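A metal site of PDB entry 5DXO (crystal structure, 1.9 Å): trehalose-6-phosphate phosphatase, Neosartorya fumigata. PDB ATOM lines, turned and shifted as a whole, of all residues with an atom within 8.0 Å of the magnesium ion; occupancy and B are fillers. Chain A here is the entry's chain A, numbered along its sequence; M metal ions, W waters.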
ATOM      1  N   PHE A  25      -9.689  -1.751   9.749  1.00  0.00           N
ATOM      2  CA  PHE A  25      -9.088  -2.605   8.728  1.00  0.00           C
ATOM      3  C   PHE A  25      -8.655  -3.947   9.316  1.00  0.00           C
ATOM      4  O   PHE A  25      -7.827  -3.982  10.202  1.00  0.00           O
ATOM      5  CB  PHE A  25      -7.840  -1.959   8.115  1.00  0.00           C
ATOM      6  CG  PHE A  25      -8.080  -0.683   7.356  1.00  0.00           C
ATOM      7  CD1 PHE A  25      -9.019  -0.616   6.357  1.00  0.00           C
ATOM      8  CD2 PHE A  25      -7.323   0.440   7.631  1.00  0.00           C
ATOM      9  CE1 PHE A  25      -9.211   0.588   5.637  1.00  0.00           C
ATOM     10  CE2 PHE A  25      -7.514   1.623   6.916  1.00  0.00           C
ATOM     11  CZ  PHE A  25      -8.454   1.700   5.940  1.00  0.00           C
ATOM     12  N   ASP A  26      -9.197  -5.047   8.801  1.00  0.00           N
ATOM     13  CA  ASP A  26      -8.505  -6.323   8.932  1.00  0.00           C
ATOM     14  C   ASP A  26      -7.113  -6.229   8.277  1.00  0.00           C
ATOM     15  O   ASP A  26      -6.908  -5.409   7.379  1.00  0.00           O
ATOM     16  CB  ASP A  26      -9.325  -7.447   8.300  1.00  0.00           C
ATOM     17  CG  ASP A  26      -8.593  -8.767   8.295  1.00  0.00           C
ATOM     18  OD1 ASP A  26      -8.172  -9.233   9.380  1.00  0.00           O
ATOM     19  OD2 ASP A  26      -8.390  -9.304   7.203  1.00  0.00           O
ATOM     20  N   TYR A  27      -6.142  -7.039   8.698  1.00  0.00           N
ATOM     21  CA  TYR A  27      -4.827  -6.959   8.066  1.00  0.00           C
ATOM     22  C   TYR A  27      -4.647  -7.987   6.935  1.00  0.00           C
ATOM     23  O   TYR A  27      -4.704  -7.630   5.760  1.00  0.00           O
ATOM     24  CB  TYR A  27      -3.698  -7.106   9.106  1.00  0.00           C
ATOM     25  CG  TYR A  27      -2.323  -6.996   8.497  1.00  0.00           C
ATOM     26  CD1 TYR A  27      -1.936  -5.874   7.783  1.00  0.00           C
ATOM     27  CD2 TYR A  27      -1.397  -8.038   8.614  1.00  0.00           C
ATOM     28  CE1 TYR A  27      -0.682  -5.774   7.202  1.00  0.00           C
ATOM     29  CE2 TYR A  27      -0.139  -7.949   8.040  1.00  0.00           C
ATOM     30  CZ  TYR A  27       0.206  -6.824   7.346  1.00  0.00           C
ATOM     31  OH  TYR A  27       1.455  -6.721   6.774  1.00  0.00           O
ATOM     32  N   ASP A  28      -4.432  -9.245   7.285  1.00  0.00           N
ATOM     33  CA  ASP A  28      -4.182 -10.302   6.287  1.00  0.00           C
ATOM     34  C   ASP A  28      -5.366 -10.562   5.354  1.00  0.00           C
ATOM     35  O   ASP A  28      -6.489 -10.835   5.806  1.00  0.00           O
ATOM     36  CB  ASP A  28      -3.779 -11.593   7.004  1.00  0.00           C
ATOM     37  CG  ASP A  28      -2.403 -11.502   7.651  1.00  0.00           C
ATOM     38  OD1 ASP A  28      -1.412 -11.323   6.902  1.00  0.00           O
ATOM     39  OD2 ASP A  28      -2.292 -11.593   8.902  1.00  0.00           O
ATOM     40  N   GLY A  29      -5.115 -10.453   4.044  1.00  0.00           N
ATOM     41  CA  GLY A  29      -6.132 -10.687   3.049  1.00  0.00           C
ATOM     42  C   GLY A  29      -6.952  -9.456   2.724  1.00  0.00           C
ATOM     43  O   GLY A  29      -7.835  -9.497   1.854  1.00  0.00           O
ATOM     44  N   THR A  30      -6.660  -8.365   3.413  1.00  0.00           N
ATOM     45  CA  THR A  30      -7.408  -7.121   3.287  1.00  0.00           C
ATOM     46  C   THR A  30      -6.480  -5.980   2.891  1.00  0.00           C
ATOM     47  O   THR A  30      -6.619  -5.373   1.837  1.00  0.00           O
ATOM     48  CB  THR A  30      -8.145  -6.788   4.596  1.00  0.00           C
ATOM     49  OG1 THR A  30      -9.071  -7.864   4.903  1.00  0.00           O
ATOM     50  CG2 THR A  30      -8.905  -5.477   4.483  1.00  0.00           C
ATOM     51  N   LEU A  31      -5.520  -5.679   3.755  1.00  0.00           N
ATOM     52  CA  LEU A  31      -4.539  -4.656   3.438  1.00  0.00           C
ATOM     53  C   LEU A  31      -3.375  -5.241   2.643  1.00  0.00           C
ATOM     54  O   LEU A  31      -2.689  -4.526   1.913  1.00  0.00           O
ATOM     55  CB  LEU A  31      -4.017  -4.013   4.710  1.00  0.00           C
ATOM     56  CG  LEU A  31      -5.019  -3.112   5.421  1.00  0.00           C
ATOM     57  CD1 LEU A  31      -4.413  -2.619   6.750  1.00  0.00           C
ATOM     58  CD2 LEU A  31      -5.427  -1.963   4.509  1.00  0.00           C
ATOM     59  N   THR A  32      -3.155  -6.538   2.818  1.00  0.00           N
ATOM     60  CA  THR A  32      -2.006  -7.208   2.219  1.00  0.00           C
ATOM     61  C   THR A  32      -2.441  -8.581   1.707  1.00  0.00           C
ATOM     62  O   THR A  32      -3.322  -9.211   2.303  1.00  0.00           O
ATOM     63  CB  THR A  32      -0.839  -7.326   3.242  1.00  0.00           C
ATOM     64  OG1 THR A  32       0.381  -7.658   2.565  1.00  0.00           O
ATOM     65  CG2 THR A  32      -1.136  -8.372   4.314  1.00  0.00           C
ATOM     66  N   ILE A  34      -2.915 -12.535   0.663  1.00  0.00           N
ATOM     67  CA  ILE A  34      -2.636 -13.852   1.222  1.00  0.00           C
ATOM     68  C   ILE A  34      -1.359 -14.397   0.573  1.00  0.00           C
ATOM     69  O   ILE A  34      -1.174 -14.276  -0.649  1.00  0.00           O
ATOM     70  CB  ILE A  34      -3.803 -14.838   0.973  1.00  0.00           C
ATOM     71  CG1 ILE A  34      -5.120 -14.287   1.542  1.00  0.00           C
ATOM     72  CG2 ILE A  34      -3.487 -16.211   1.559  1.00  0.00           C
ATOM     73  CD1 ILE A  34      -5.229 -14.369   3.072  1.00  0.00           C
ATOM     74  N   ILE A  65      -6.825  -4.355  12.843  1.00  0.00           N
ATOM     75  CA  ILE A  65      -7.394  -5.403  13.685  1.00  0.00           C
ATOM     76  C   ILE A  65      -6.910  -6.747  13.159  1.00  0.00           C
ATOM     77  O   ILE A  65      -7.206  -7.113  12.021  1.00  0.00           O
ATOM     78  CB  ILE A  65      -8.912  -5.319  13.683  1.00  0.00           C
ATOM     79  CG1 ILE A  65      -9.312  -3.861  13.992  1.00  0.00           C
ATOM     80  CG2 ILE A  65      -9.519  -6.324  14.675  1.00  0.00           C
ATOM     81  CD1 ILE A  65     -10.784  -3.636  14.065  1.00  0.00           C
ATOM     82  N   SER A  66      -6.117  -7.459  13.966  1.00  0.00           N
ATOM     83  CA  SER A  66      -5.363  -8.604  13.449  1.00  0.00           C
ATOM     84  C   SER A  66      -5.191  -9.734  14.463  1.00  0.00           C
ATOM     85  O   SER A  66      -5.220  -9.496  15.662  1.00  0.00           O
ATOM     86  CB  SER A  66      -3.991  -8.113  12.973  1.00  0.00           C
ATOM     87  OG  SER A  66      -3.200  -9.177  12.500  1.00  0.00           O
ATOM     88  N   GLY A  67      -5.016 -10.956  13.963  1.00  0.00           N
ATOM     89  CA  GLY A  67      -4.711 -12.088  14.810  1.00  0.00           C
ATOM     90  C   GLY A  67      -3.229 -12.145  15.155  1.00  0.00           C
ATOM     91  O   GLY A  67      -2.804 -12.884  16.057  1.00  0.00           O
ATOM     92  N   LYS A 190     -14.483 -10.261  16.715  1.00  0.00           N
ATOM     93  CA  LYS A 190     -14.260  -9.026  15.958  1.00  0.00           C
ATOM     94  C   LYS A 190     -15.468  -8.088  15.976  1.00  0.00           C
ATOM     95  O   LYS A 190     -15.295  -6.871  15.875  1.00  0.00           O
ATOM     96  CB  LYS A 190     -13.871  -9.347  14.523  1.00  0.00           C
ATOM     97  CG  LYS A 190     -12.398  -9.163  14.242  1.00  0.00           C
ATOM     98  CD  LYS A 190     -12.095  -9.291  12.737  1.00  0.00           C
ATOM     99  CE  LYS A 190     -10.601  -9.199  12.455  1.00  0.00           C
ATOM    100  NZ  LYS A 190     -10.260  -9.695  11.077  1.00  0.00           N
ATOM    101  N   LEU A 215     -13.466  -2.936   6.772  1.00  0.00           N
ATOM    102  CA  LEU A 215     -13.007  -3.823   5.695  1.00  0.00           C
ATOM    103  C   LEU A 215     -12.432  -5.150   6.181  1.00  0.00           C
ATOM    104  O   LEU A 215     -11.573  -5.153   7.044  1.00  0.00           O
ATOM    105  CB  LEU A 215     -11.930  -3.110   4.894  1.00  0.00           C
ATOM    106  CG  LEU A 215     -12.353  -2.049   3.893  1.00  0.00           C
ATOM    107  CD1 LEU A 215     -11.210  -1.119   3.713  1.00  0.00           C
ATOM    108  CD2 LEU A 215     -12.634  -2.725   2.588  1.00  0.00           C
ATOM    109  N   GLY A 216     -12.832  -6.257   5.568  1.00  0.00           N
ATOM    110  CA  GLY A 216     -12.278  -7.553   5.944  1.00  0.00           C
ATOM    111  C   GLY A 216     -12.588  -8.607   4.896  1.00  0.00           C
ATOM    112  O   GLY A 216     -13.470  -8.395   4.079  1.00  0.00           O
ATOM    113  N   ASP A 217     -11.873  -9.730   4.920  1.00  0.00           N
ATOM    114  CA  ASP A 217     -11.915 -10.689   3.816  1.00  0.00           C
ATOM    115  C   ASP A 217     -12.487 -12.064   4.157  1.00  0.00           C
ATOM    116  O   ASP A 217     -12.772 -12.855   3.252  1.00  0.00           O
ATOM    117  CB  ASP A 217     -10.510 -10.867   3.233  1.00  0.00           C
ATOM    118  CG  ASP A 217      -9.569 -11.583   4.186  1.00  0.00           C
ATOM    119  OD1 ASP A 217      -9.388 -11.090   5.311  1.00  0.00           O
ATOM    120  OD2 ASP A 217      -9.006 -12.640   3.798  1.00  0.00           O
ATOM    121  N   ASP A 218     -12.660 -12.404   5.427  1.00  0.00           N
ATOM    122  CA  ASP A 218     -13.238 -13.732   5.665  1.00  0.00           C
ATOM    123  C   ASP A 218     -14.327 -13.775   6.699  1.00  0.00           C
ATOM    124  O   ASP A 218     -14.905 -12.754   7.072  1.00  0.00           O
ATOM    125  CB  ASP A 218     -12.134 -14.738   6.027  1.00  0.00           C
ATOM    126  CG  ASP A 218     -11.401 -14.395   7.294  1.00  0.00           C
ATOM    127  OD1 ASP A 218     -11.944 -13.697   8.168  1.00  0.00           O
ATOM    128  OD2 ASP A 218     -10.244 -14.841   7.424  1.00  0.00           O
ATOM    129  N   PHE A 219     -14.610 -14.993   7.172  1.00  0.00           N
ATOM    130  CA  PHE A 219     -15.759 -15.213   8.031  1.00  0.00           C
ATOM    131  C   PHE A 219     -15.608 -14.522   9.388  1.00  0.00           C
ATOM    132  O   PHE A 219     -16.605 -14.196  10.002  1.00  0.00           O
ATOM    133  CB  PHE A 219     -16.000 -16.736   8.205  1.00  0.00           C
ATOM    134  CG  PHE A 219     -14.879 -17.468   8.877  1.00  0.00           C
ATOM    135  CD1 PHE A 219     -14.947 -17.784  10.228  1.00  0.00           C
ATOM    136  CD2 PHE A 219     -13.751 -17.872   8.164  1.00  0.00           C
ATOM    137  CE1 PHE A 219     -13.918 -18.482  10.864  1.00  0.00           C
ATOM    138  CE2 PHE A 219     -12.723 -18.569   8.785  1.00  0.00           C
ATOM    139  CZ  PHE A 219     -12.807 -18.869  10.147  1.00  0.00           C
ATOM    140  N   THR A 220     -14.385 -14.265   9.838  1.00  0.00           N
ATOM    141  CA  THR A 220     -14.209 -13.582  11.127  1.00  0.00           C
ATOM    142  C   THR A 220     -14.607 -12.105  11.059  1.00  0.00           C
ATOM    143  O   THR A 220     -15.004 -11.495  12.045  1.00  0.00           O
ATOM    144  CB  THR A 220     -12.771 -13.681  11.639  1.00  0.00           C
ATOM    145  OG1 THR A 220     -11.903 -12.911  10.775  1.00  0.00           O
ATOM    146  CG2 THR A 220     -12.323 -15.142  11.652  1.00  0.00           C
ATOM    147  N   ASP A 221     -14.501 -11.541   9.863  1.00  0.00           N
ATOM    148  CA  ASP A 221     -14.874 -10.155   9.621  1.00  0.00           C
ATOM    149  C   ASP A 221     -16.381  -9.944   9.497  1.00  0.00           C
ATOM    150  O   ASP A 221     -16.897  -8.870   9.801  1.00  0.00           O
ATOM    151  CB  ASP A 221     -14.152  -9.663   8.356  1.00  0.00           C
ATOM    152  CG  ASP A 221     -12.658  -9.889   8.437  1.00  0.00           C
ATOM    153  OD1 ASP A 221     -12.021  -9.280   9.335  1.00  0.00           O
ATOM    154  OD2 ASP A 221     -12.116 -10.684   7.635  1.00  0.00           O
ATOM    155  N   VAL A 243     -13.755  -8.062   1.109  1.00  0.00           N
ATOM    156  CA  VAL A 243     -12.782  -8.210   0.061  1.00  0.00           C
ATOM    157  C   VAL A 243     -12.965  -9.598  -0.555  1.00  0.00           C
ATOM    158  O   VAL A 243     -12.732 -10.613   0.088  1.00  0.00           O
ATOM    159  CB  VAL A 243     -11.350  -8.051   0.570  1.00  0.00           C
ATOM    160  CG1 VAL A 243     -10.395  -8.083  -0.618  1.00  0.00           C
ATOM    161  CG2 VAL A 243     -11.206  -6.706   1.331  1.00  0.00           C
HETATM  162 MG    MG M   1      -8.031 -11.365   6.907  1.00  0.00          MG
HETATM  163  O   HOH W   1      -7.016 -11.605   8.662  1.00  0.00           O
HETATM  164  O   HOH W   2      -7.911 -13.408   6.385  1.00  0.00           O
HETATM  165  O   HOH W   3      -9.751 -11.506   7.815  1.00  0.00           O
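The backbone NH (N) of Asp 217 lies within hydrogen-bond range of the side-chain hydroxyl (OG1) of Thr 30 (3.4 Å).
The backbone NH (N) of Asp 217 lies within hydrogen-bond range of the side-chain carboxylate (OD2) of Asp 221, at 2.9 Å.
The side-chain carboxylate (OD2) of Asp 26 sits close to the side-chain hydroxyl (OG1) of Thr 30.
The side-chain amino group (NZ) of Lys 190 lies within salt-bridge range of the side-chain carboxylate (OD1) of Asp 26, 2.7 Å away.
The backbone NH of Asp 26 lies within hydrogen-bond range of the backbone carbonyl oxygen of Leu 215 (3.0 Å).
Within 4 Å of the magnesium ion: Asp 26, Asp 28 and Asp 217.
The nearest printed residue that does not touch the magnesium ion is Asp 218 (4.2 Å).
The magnesium ion is bound by water W3, O of Asp 28, water W1, water W2, OD1 of Asp 217 and OD2 of Asp 26.
Water W2 bridges the side-chain carboxylate (OD2) of Asp 217 (2.9 Å) and the side-chain carboxylate (OD2) of Asp 218 (2.9 Å).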
